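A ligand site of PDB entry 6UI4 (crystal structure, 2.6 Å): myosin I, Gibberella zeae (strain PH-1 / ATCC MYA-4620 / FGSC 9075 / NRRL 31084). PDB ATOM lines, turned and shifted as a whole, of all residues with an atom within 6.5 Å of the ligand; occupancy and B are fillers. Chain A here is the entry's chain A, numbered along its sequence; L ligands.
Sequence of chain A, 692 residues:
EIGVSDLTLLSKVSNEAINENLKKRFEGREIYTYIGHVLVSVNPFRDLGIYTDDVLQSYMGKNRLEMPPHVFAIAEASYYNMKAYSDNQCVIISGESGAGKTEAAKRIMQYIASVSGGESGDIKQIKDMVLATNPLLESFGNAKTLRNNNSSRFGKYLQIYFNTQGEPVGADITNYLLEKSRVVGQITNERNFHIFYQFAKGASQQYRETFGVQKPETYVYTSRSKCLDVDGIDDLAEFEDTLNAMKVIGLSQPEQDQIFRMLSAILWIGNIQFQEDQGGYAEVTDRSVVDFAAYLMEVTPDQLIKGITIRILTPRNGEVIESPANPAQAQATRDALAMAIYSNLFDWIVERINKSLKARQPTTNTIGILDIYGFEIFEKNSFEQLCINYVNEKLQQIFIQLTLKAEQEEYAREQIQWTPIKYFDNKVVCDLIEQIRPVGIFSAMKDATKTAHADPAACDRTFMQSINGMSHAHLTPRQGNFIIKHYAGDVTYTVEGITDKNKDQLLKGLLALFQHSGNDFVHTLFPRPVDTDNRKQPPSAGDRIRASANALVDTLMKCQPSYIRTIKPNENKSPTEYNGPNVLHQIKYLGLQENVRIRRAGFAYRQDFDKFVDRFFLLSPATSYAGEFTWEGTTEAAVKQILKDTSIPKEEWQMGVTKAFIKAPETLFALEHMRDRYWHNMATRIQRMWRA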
ATOM      1  N   ARG A 153      10.426  29.917 -15.795  1.00  0.00           N
ATOM      2  CA  ARG A 153      11.394  29.666 -16.843  1.00  0.00           C
ATOM      3  C   ARG A 153      11.412  30.783 -17.873  1.00  0.00           C
ATOM      4  O   ARG A 153      11.914  30.606 -18.990  1.00  0.00           O
ATOM      5  CB  ARG A 153      11.122  28.332 -17.554  1.00  0.00           C
ATOM      6  CG  ARG A 153      10.994  27.111 -16.668  1.00  0.00           C
ATOM      7  CD  ARG A 153      12.081  26.989 -15.619  1.00  0.00           C
ATOM      8  NE  ARG A 153      13.427  26.872 -16.179  1.00  0.00           N
ATOM      9  CZ  ARG A 153      14.531  27.052 -15.466  1.00  0.00           C
ATOM     10  NH1 ARG A 153      14.448  27.320 -14.169  1.00  0.00           N
ATOM     11  NH2 ARG A 153      15.725  26.950 -16.031  1.00  0.00           N
ATOM     12  N   PHE A 154      10.858  31.934 -17.519  1.00  0.00           N
ATOM     13  CA  PHE A 154      10.856  33.130 -18.333  1.00  0.00           C
ATOM     14  C   PHE A 154      10.930  34.322 -17.392  1.00  0.00           C
ATOM     15  O   PHE A 154      10.589  34.214 -16.214  1.00  0.00           O
ATOM     16  CB  PHE A 154       9.607  33.203 -19.218  1.00  0.00           C
ATOM     17  CG  PHE A 154       8.343  33.512 -18.462  1.00  0.00           C
ATOM     18  CD1 PHE A 154       7.744  34.765 -18.566  1.00  0.00           C
ATOM     19  CD2 PHE A 154       7.781  32.567 -17.621  1.00  0.00           C
ATOM     20  CE1 PHE A 154       6.587  35.050 -17.856  1.00  0.00           C
ATOM     21  CE2 PHE A 154       6.633  32.850 -16.900  1.00  0.00           C
ATOM     22  CZ  PHE A 154       6.037  34.098 -17.025  1.00  0.00           C
ATOM     23  N   LEU A 177      13.652  36.091 -22.434  1.00  0.00           N
ATOM     24  CA  LEU A 177      13.834  34.838 -23.162  1.00  0.00           C
ATOM     25  C   LEU A 177      13.344  33.631 -22.369  1.00  0.00           C
ATOM     26  O   LEU A 177      13.744  33.435 -21.216  1.00  0.00           O
ATOM     27  CB  LEU A 177      15.309  34.651 -23.537  1.00  0.00           C
ATOM     28  CG  LEU A 177      15.799  35.268 -24.857  1.00  0.00           C
ATOM     29  CD1 LEU A 177      15.474  36.746 -24.931  1.00  0.00           C
ATOM     30  CD2 LEU A 177      17.288  35.030 -25.025  1.00  0.00           C
ATOM     31  N   LEU A 178      12.494  32.833 -22.993  1.00  0.00           N
ATOM     32  CA  LEU A 178      11.941  31.613 -22.409  1.00  0.00           C
ATOM     33  C   LEU A 178      12.865  30.421 -22.644  1.00  0.00           C
ATOM     34  O   LEU A 178      13.562  30.343 -23.660  1.00  0.00           O
ATOM     35  CB  LEU A 178      10.564  31.342 -23.024  1.00  0.00           C
ATOM     36  CG  LEU A 178       9.897  29.987 -22.791  1.00  0.00           C
ATOM     37  CD1 LEU A 178       9.236  29.956 -21.414  1.00  0.00           C
ATOM     38  CD2 LEU A 178       8.896  29.683 -23.888  1.00  0.00           C
ATOM     39  N   GLU A 179      12.880  29.497 -21.675  1.00  0.00           N
ATOM     40  CA  GLU A 179      13.667  28.265 -21.781  1.00  0.00           C
ATOM     41  C   GLU A 179      12.936  27.250 -22.665  1.00  0.00           C
ATOM     42  O   GLU A 179      12.373  26.256 -22.201  1.00  0.00           O
ATOM     43  CB  GLU A 179      13.955  27.684 -20.398  1.00  0.00           C
ATOM     44  CG  GLU A 179      14.960  26.535 -20.415  1.00  0.00           C
ATOM     45  CD  GLU A 179      14.974  25.709 -19.139  1.00  0.00           C
ATOM     46  OE1 GLU A 179      13.953  25.708 -18.413  1.00  0.00           O
ATOM     47  OE2 GLU A 179      15.992  25.044 -18.862  1.00  0.00           O
ATOM     48  N   LYS A 180      12.959  27.510 -23.978  1.00  0.00           N
ATOM     49  CA  LYS A 180      12.233  26.655 -24.924  1.00  0.00           C
ATOM     50  C   LYS A 180      12.757  25.225 -24.916  1.00  0.00           C
ATOM     51  O   LYS A 180      11.999  24.288 -25.211  1.00  0.00           O
ATOM     52  CB  LYS A 180      12.301  27.251 -26.332  1.00  0.00           C
ATOM     53  CG  LYS A 180      13.480  28.178 -26.560  1.00  0.00           C
ATOM     54  CD  LYS A 180      13.554  28.677 -27.993  1.00  0.00           C
ATOM     55  CE  LYS A 180      14.131  27.620 -28.923  1.00  0.00           C
ATOM     56  NZ  LYS A 180      14.473  28.203 -30.259  1.00  0.00           N
ATOM     57  N   SER A 181      14.026  25.017 -24.553  1.00  0.00           N
ATOM     58  CA  SER A 181      14.624  23.694 -24.665  1.00  0.00           C
ATOM     59  C   SER A 181      13.912  22.702 -23.751  1.00  0.00           C
ATOM     60  O   SER A 181      13.846  21.506 -24.058  1.00  0.00           O
ATOM     61  CB  SER A 181      16.122  23.753 -24.329  1.00  0.00           C
ATOM     62  OG  SER A 181      16.314  24.204 -23.003  1.00  0.00           O
ATOM     63  N   ARG A 182      13.374  23.198 -22.639  1.00  0.00           N
ATOM     64  CA  ARG A 182      12.587  22.387 -21.718  1.00  0.00           C
ATOM     65  C   ARG A 182      11.564  21.542 -22.479  1.00  0.00           C
ATOM     66  O   ARG A 182      11.334  20.371 -22.145  1.00  0.00           O
ATOM     67  CB  ARG A 182      11.902  23.305 -20.713  1.00  0.00           C
ATOM     68  CG  ARG A 182      10.834  22.686 -19.840  1.00  0.00           C
ATOM     69  CD  ARG A 182      11.366  22.211 -18.492  1.00  0.00           C
ATOM     70  NE  ARG A 182      12.341  23.121 -17.918  1.00  0.00           N
ATOM     71  CZ  ARG A 182      13.264  22.752 -17.036  1.00  0.00           C
ATOM     72  NH1 ARG A 182      13.270  21.509 -16.566  1.00  0.00           N
ATOM     73  NH2 ARG A 182      14.132  23.631 -16.566  1.00  0.00           N
ATOM     74  N   MET A 339      10.487  23.205 -30.422  1.00  0.00           N
ATOM     75  CA  MET A 339      10.868  24.399 -29.670  1.00  0.00           C
ATOM     76  C   MET A 339      10.365  25.659 -30.354  1.00  0.00           C
ATOM     77  O   MET A 339       9.893  26.588 -29.673  1.00  0.00           O
ATOM     78  CB  MET A 339      12.390  24.464 -29.517  1.00  0.00           C
ATOM     79  CG  MET A 339      12.958  23.621 -28.385  1.00  0.00           C
ATOM     80  SD  MET A 339      14.748  23.830 -28.297  1.00  0.00           S
ATOM     81  CE  MET A 339      15.307  22.571 -29.448  1.00  0.00           C
ATOM     82  N   TYR A 373      13.698  35.166 -13.586  1.00  0.00           N
ATOM     83  CA  TYR A 373      14.108  33.849 -13.106  1.00  0.00           C
ATOM     84  C   TYR A 373      15.367  34.005 -12.264  1.00  0.00           C
ATOM     85  O   TYR A 373      16.313  34.697 -12.676  1.00  0.00           O
ATOM     86  CB  TYR A 373      14.329  32.861 -14.259  1.00  0.00           C
ATOM     87  CG  TYR A 373      14.608  33.423 -15.651  1.00  0.00           C
ATOM     88  CD1 TYR A 373      15.292  34.622 -15.838  1.00  0.00           C
ATOM     89  CD2 TYR A 373      14.164  32.754 -16.783  1.00  0.00           C
ATOM     90  CE1 TYR A 373      15.525  35.129 -17.104  1.00  0.00           C
ATOM     91  CE2 TYR A 373      14.399  33.254 -18.061  1.00  0.00           C
ATOM     92  CZ  TYR A 373      15.078  34.444 -18.210  1.00  0.00           C
ATOM     93  OH  TYR A 373      15.330  34.948 -19.463  1.00  0.00           O
ATOM     94  N   PHE A 383      23.867  27.355 -22.118  1.00  0.00           N
ATOM     95  CA  PHE A 383      23.393  28.709 -22.429  1.00  0.00           C
ATOM     96  C   PHE A 383      22.212  29.138 -21.560  1.00  0.00           C
ATOM     97  O   PHE A 383      22.161  30.295 -21.121  1.00  0.00           O
ATOM     98  CB  PHE A 383      22.996  28.819 -23.896  1.00  0.00           C
ATOM     99  CG  PHE A 383      22.862  30.237 -24.347  1.00  0.00           C
ATOM    100  CD1 PHE A 383      23.976  30.954 -24.742  1.00  0.00           C
ATOM    101  CD2 PHE A 383      21.640  30.888 -24.288  1.00  0.00           C
ATOM    102  CE1 PHE A 383      23.866  32.285 -25.129  1.00  0.00           C
ATOM    103  CE2 PHE A 383      21.529  32.217 -24.666  1.00  0.00           C
ATOM    104  CZ  PHE A 383      22.647  32.910 -25.087  1.00  0.00           C
ATOM    105  N   GLU A 384      21.213  28.271 -21.408  1.00  0.00           N
ATOM    106  CA  GLU A 384      20.033  28.625 -20.609  1.00  0.00           C
ATOM    107  C   GLU A 384      20.433  29.263 -19.282  1.00  0.00           C
ATOM    108  O   GLU A 384      19.992  30.373 -18.946  1.00  0.00           O
ATOM    109  CB  GLU A 384      19.199  27.366 -20.341  1.00  0.00           C
ATOM    110  CG  GLU A 384      18.544  26.774 -21.574  1.00  0.00           C
ATOM    111  CD  GLU A 384      19.417  25.713 -22.219  1.00  0.00           C
ATOM    112  OE1 GLU A 384      20.656  25.772 -22.061  1.00  0.00           O
ATOM    113  OE2 GLU A 384      18.857  24.808 -22.886  1.00  0.00           O
ATOM    114  N   GLN A 385      21.290  28.566 -18.545  1.00  0.00           N
ATOM    115  CA  GLN A 385      21.738  29.028 -17.246  1.00  0.00           C
ATOM    116  C   GLN A 385      22.606  30.278 -17.388  1.00  0.00           C
ATOM    117  O   GLN A 385      22.575  31.140 -16.514  1.00  0.00           O
ATOM    118  CB  GLN A 385      22.478  27.899 -16.542  1.00  0.00           C
ATOM    119  CG  GLN A 385      21.516  26.937 -15.880  1.00  0.00           C
ATOM    120  CD  GLN A 385      20.931  25.950 -16.883  1.00  0.00           C
ATOM    121  OE1 GLN A 385      21.542  25.639 -17.897  1.00  0.00           O
ATOM    122  NE2 GLN A 385      19.715  25.495 -16.610  1.00  0.00           N
ATOM    123  N   CYS A 387      22.237  32.666 -19.614  1.00  0.00           N
ATOM    124  CA  CYS A 387      21.314  33.777 -19.837  1.00  0.00           C
ATOM    125  C   CYS A 387      20.632  34.175 -18.529  1.00  0.00           C
ATOM    126  O   CYS A 387      20.579  35.361 -18.166  1.00  0.00           O
ATOM    127  CB  CYS A 387      20.301  33.382 -20.907  1.00  0.00           C
ATOM    128  SG  CYS A 387      18.808  34.388 -20.998  1.00  0.00           S
ATOM    129  N   ILE A 388      20.116  33.169 -17.802  1.00  0.00           N
ATOM    130  CA  ILE A 388      19.422  33.443 -16.537  1.00  0.00           C
ATOM    131  C   ILE A 388      20.369  34.113 -15.550  1.00  0.00           C
ATOM    132  O   ILE A 388      20.022  35.132 -14.913  1.00  0.00           O
ATOM    133  CB  ILE A 388      18.824  32.134 -15.982  1.00  0.00           C
ATOM    134  CG1 ILE A 388      17.692  31.654 -16.902  1.00  0.00           C
ATOM    135  CG2 ILE A 388      18.362  32.328 -14.554  1.00  0.00           C
ATOM    136  CD1 ILE A 388      17.026  30.379 -16.450  1.00  0.00           C
ATOM    137  N   ASP A 500      25.413  26.792 -30.706  1.00  0.00           N
ATOM    138  CA  ASP A 500      24.184  26.607 -31.467  1.00  0.00           C
ATOM    139  C   ASP A 500      23.001  27.149 -30.673  1.00  0.00           C
ATOM    140  O   ASP A 500      22.103  27.771 -31.247  1.00  0.00           O
ATOM    141  CB  ASP A 500      23.990  25.137 -31.820  1.00  0.00           C
ATOM    142  CG  ASP A 500      23.024  24.952 -32.975  1.00  0.00           C
ATOM    143  OD1 ASP A 500      23.284  25.509 -34.068  1.00  0.00           O
ATOM    144  OD2 ASP A 500      22.018  24.233 -32.797  1.00  0.00           O
ATOM    145  N   LYS A 501      22.977  26.899 -29.357  1.00  0.00           N
ATOM    146  CA  LYS A 501      21.976  27.538 -28.504  1.00  0.00           C
ATOM    147  C   LYS A 501      22.011  29.051 -28.639  1.00  0.00           C
ATOM    148  O   LYS A 501      20.962  29.704 -28.673  1.00  0.00           O
ATOM    149  CB  LYS A 501      22.189  27.130 -27.043  1.00  0.00           C
ATOM    150  CG  LYS A 501      21.915  25.668 -26.707  1.00  0.00           C
ATOM    151  CD  LYS A 501      22.151  25.430 -25.220  1.00  0.00           C
ATOM    152  CE  LYS A 501      21.947  23.981 -24.798  1.00  0.00           C
ATOM    153  NZ  LYS A 501      20.522  23.604 -24.635  1.00  0.00           N
ATOM    154  N   ASN A 502      23.208  29.640 -28.713  1.00  0.00           N
ATOM    155  CA  ASN A 502      23.293  31.091 -28.837  1.00  0.00           C
ATOM    156  C   ASN A 502      22.826  31.537 -30.215  1.00  0.00           C
ATOM    157  O   ASN A 502      22.134  32.553 -30.340  1.00  0.00           O
ATOM    158  CB  ASN A 502      24.712  31.590 -28.585  1.00  0.00           C
ATOM    159  CG  ASN A 502      24.863  33.076 -28.837  1.00  0.00           C
ATOM    160  OD1 ASN A 502      24.262  33.902 -28.147  1.00  0.00           O
ATOM    161  ND2 ASN A 502      25.653  33.427 -29.855  1.00  0.00           N
ATOM    162  N   LYS A 503      23.197  30.794 -31.246  1.00  0.00           N
ATOM    163  CA  LYS A 503      22.724  31.009 -32.612  1.00  0.00           C
ATOM    164  C   LYS A 503      21.353  30.348 -32.744  1.00  0.00           C
ATOM    165  O   LYS A 503      21.214  29.204 -33.192  1.00  0.00           O
ATOM    166  CB  LYS A 503      23.713  30.437 -33.615  1.00  0.00           C
ATOM    167  CG  LYS A 503      23.195  30.314 -35.042  1.00  0.00           C
ATOM    168  CD  LYS A 503      24.116  29.423 -35.856  1.00  0.00           C
ATOM    169  CE  LYS A 503      23.575  29.166 -37.248  1.00  0.00           C
ATOM    170  NZ  LYS A 503      24.543  28.365 -38.042  1.00  0.00           N
ATOM    171  N   ASP A 504      20.316  31.066 -32.333  1.00  0.00           N
ATOM    172  CA  ASP A 504      18.996  30.442 -32.231  1.00  0.00           C
ATOM    173  C   ASP A 504      18.293  30.737 -33.553  1.00  0.00           C
ATOM    174  O   ASP A 504      17.462  31.631 -33.674  1.00  0.00           O
ATOM    175  CB  ASP A 504      18.224  30.976 -31.034  1.00  0.00           C
ATOM    176  CG  ASP A 504      16.848  30.339 -30.890  1.00  0.00           C
ATOM    177  OD1 ASP A 504      16.651  29.228 -31.441  1.00  0.00           O
ATOM    178  OD2 ASP A 504      15.982  30.941 -30.228  1.00  0.00           O
ATOM    179  N   GLN A 505      18.674  29.972 -34.577  1.00  0.00           N
ATOM    180  CA  GLN A 505      18.239  30.239 -35.935  1.00  0.00           C
ATOM    181  C   GLN A 505      17.659  28.976 -36.541  1.00  0.00           C
ATOM    182  O   GLN A 505      18.307  27.928 -36.545  1.00  0.00           O
ATOM    183  CB  GLN A 505      19.394  30.782 -36.775  1.00  0.00           C
ATOM    184  CG  GLN A 505      19.077  30.959 -38.246  1.00  0.00           C
ATOM    185  CD  GLN A 505      20.288  31.399 -39.033  1.00  0.00           C
ATOM    186  OE1 GLN A 505      21.134  32.131 -38.520  1.00  0.00           O
ATOM    187  NE2 GLN A 505      20.379  30.966 -40.288  1.00  0.00           N
ATOM    188  N   ALA A 541      20.658  34.926 -29.462  1.00  0.00           N
ATOM    189  CA  ALA A 541      19.928  35.003 -28.201  1.00  0.00           C
ATOM    190  C   ALA A 541      20.638  35.917 -27.211  1.00  0.00           C
ATOM    191  O   ALA A 541      19.998  36.638 -26.438  1.00  0.00           O
ATOM    192  CB  ALA A 541      19.739  33.611 -27.596  1.00  0.00           C
ATOM    193  N   GLY A 542      21.981  35.901 -27.226  1.00  0.00           N
ATOM    194  CA  GLY A 542      22.724  36.759 -26.329  1.00  0.00           C
ATOM    195  C   GLY A 542      22.546  38.221 -26.681  1.00  0.00           C
ATOM    196  O   GLY A 542      22.483  39.078 -25.791  1.00  0.00           O
HETATM  197  C1  LIG L   1      18.352  25.605 -27.143  1.00  0.00           C
HETATM  198  C2  LIG L   1      17.510  30.541 -23.880  1.00  0.00           C
HETATM  199  C3  LIG L   1      17.385  31.236 -21.625  1.00  0.00           C
HETATM  200  C4  LIG L   1      16.421  31.315 -20.423  1.00  0.00           C
HETATM  201  C5  LIG L   1      18.372  26.730 -26.319  1.00  0.00           C
HETATM  202  C6  LIG L   1      18.122  25.750 -28.507  1.00  0.00           C
HETATM  203  C7  LIG L   1      18.132  28.000 -26.863  1.00  0.00           C
HETATM  204  C8  LIG L   1      17.914  27.013 -29.059  1.00  0.00           C
HETATM  205  C9  LIG L   1      17.924  28.139 -28.236  1.00  0.00           C
HETATM  206  C10 LIG L   1      18.160  29.252 -25.964  1.00  0.00           C
HETATM  207  C11 LIG L   1      17.462  29.289 -24.782  1.00  0.00           C
HETATM  208  C12 LIG L   1      16.616  28.092 -24.353  1.00  0.00           C
HETATM  209  N1  LIG L   1      15.989  27.203 -24.036  1.00  0.00           N
HETATM  210  N2  LIG L   1      18.985  30.434 -26.378  1.00  0.00           N
HETATM  211  O1  LIG L   1      18.144  31.500 -24.188  1.00  0.00           O
HETATM  212  O2  LIG L   1      16.760  30.561 -22.688  1.00  0.00           O
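The backbone NH of Ser 181 sits at hydrogen-bond distance from a nitrogen (N1) of the ligand (3.0 Å). OG of Ser 181 sits at hydrogen-bond distance from N1 of the ligand. N of Lys 180 is in hydrogen-bond range of N1 of the ligand, at 3.0 Å. A nitrogen (N2) of the ligand sits at hydrogen-bond distance from the backbone carbonyl oxygen (O) of Lys 501.
The side-chain hydroxyl (OG) of Ser 181 is in hydrogen-bond range of the side-chain carboxylate (OE2) of Glu 384 (2.6 Å). NZ of Lys 180 lies within salt-bridge range of OD1 of Asp 504, 2.7 Å away. NZ of Lys 501 lies within salt-bridge range of OE2 of Glu 384 (2.7 Å). The side-chain carboxylate (OE1) of Glu 179 is in salt-bridge range of the guanidinium group (NE) of Arg 153 (2.6 Å). OE1 of Glu 179 lies within salt-bridge range of NH2 of Arg 182 (2.8 Å). The backbone carbonyl oxygen (O) of Asn 502 is in hydrogen-bond range of the backbone NH (N) of Ala 541, at 2.9 Å. O of Leu 177 sits at hydrogen-bond distance from OH of Tyr 373 (2.8 Å).
An oxygen (O2) of the ligand lies close to the backbone carbonyl oxygen (O) of Leu 178 (3.3 Å). Merely in contact with the ligand: Glu 179 (3.3 Å), Phe 383 (3.4 Å), Ala 541 (3.5 Å), Asp 504 (3.5 Å), Leu 177 (3.5 Å), Cys 387 (3.5 Å), Glu 384 (3.6 Å), Tyr 373 (3.7 Å), Ile 388 (3.8 Å) and Met 339 (3.9 Å). Hydrophobic or aromatic side chains within 4 Å of the ligand: Leu 177, Met 339, Tyr 373, Phe 383, Ile 388 and Ala 541.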
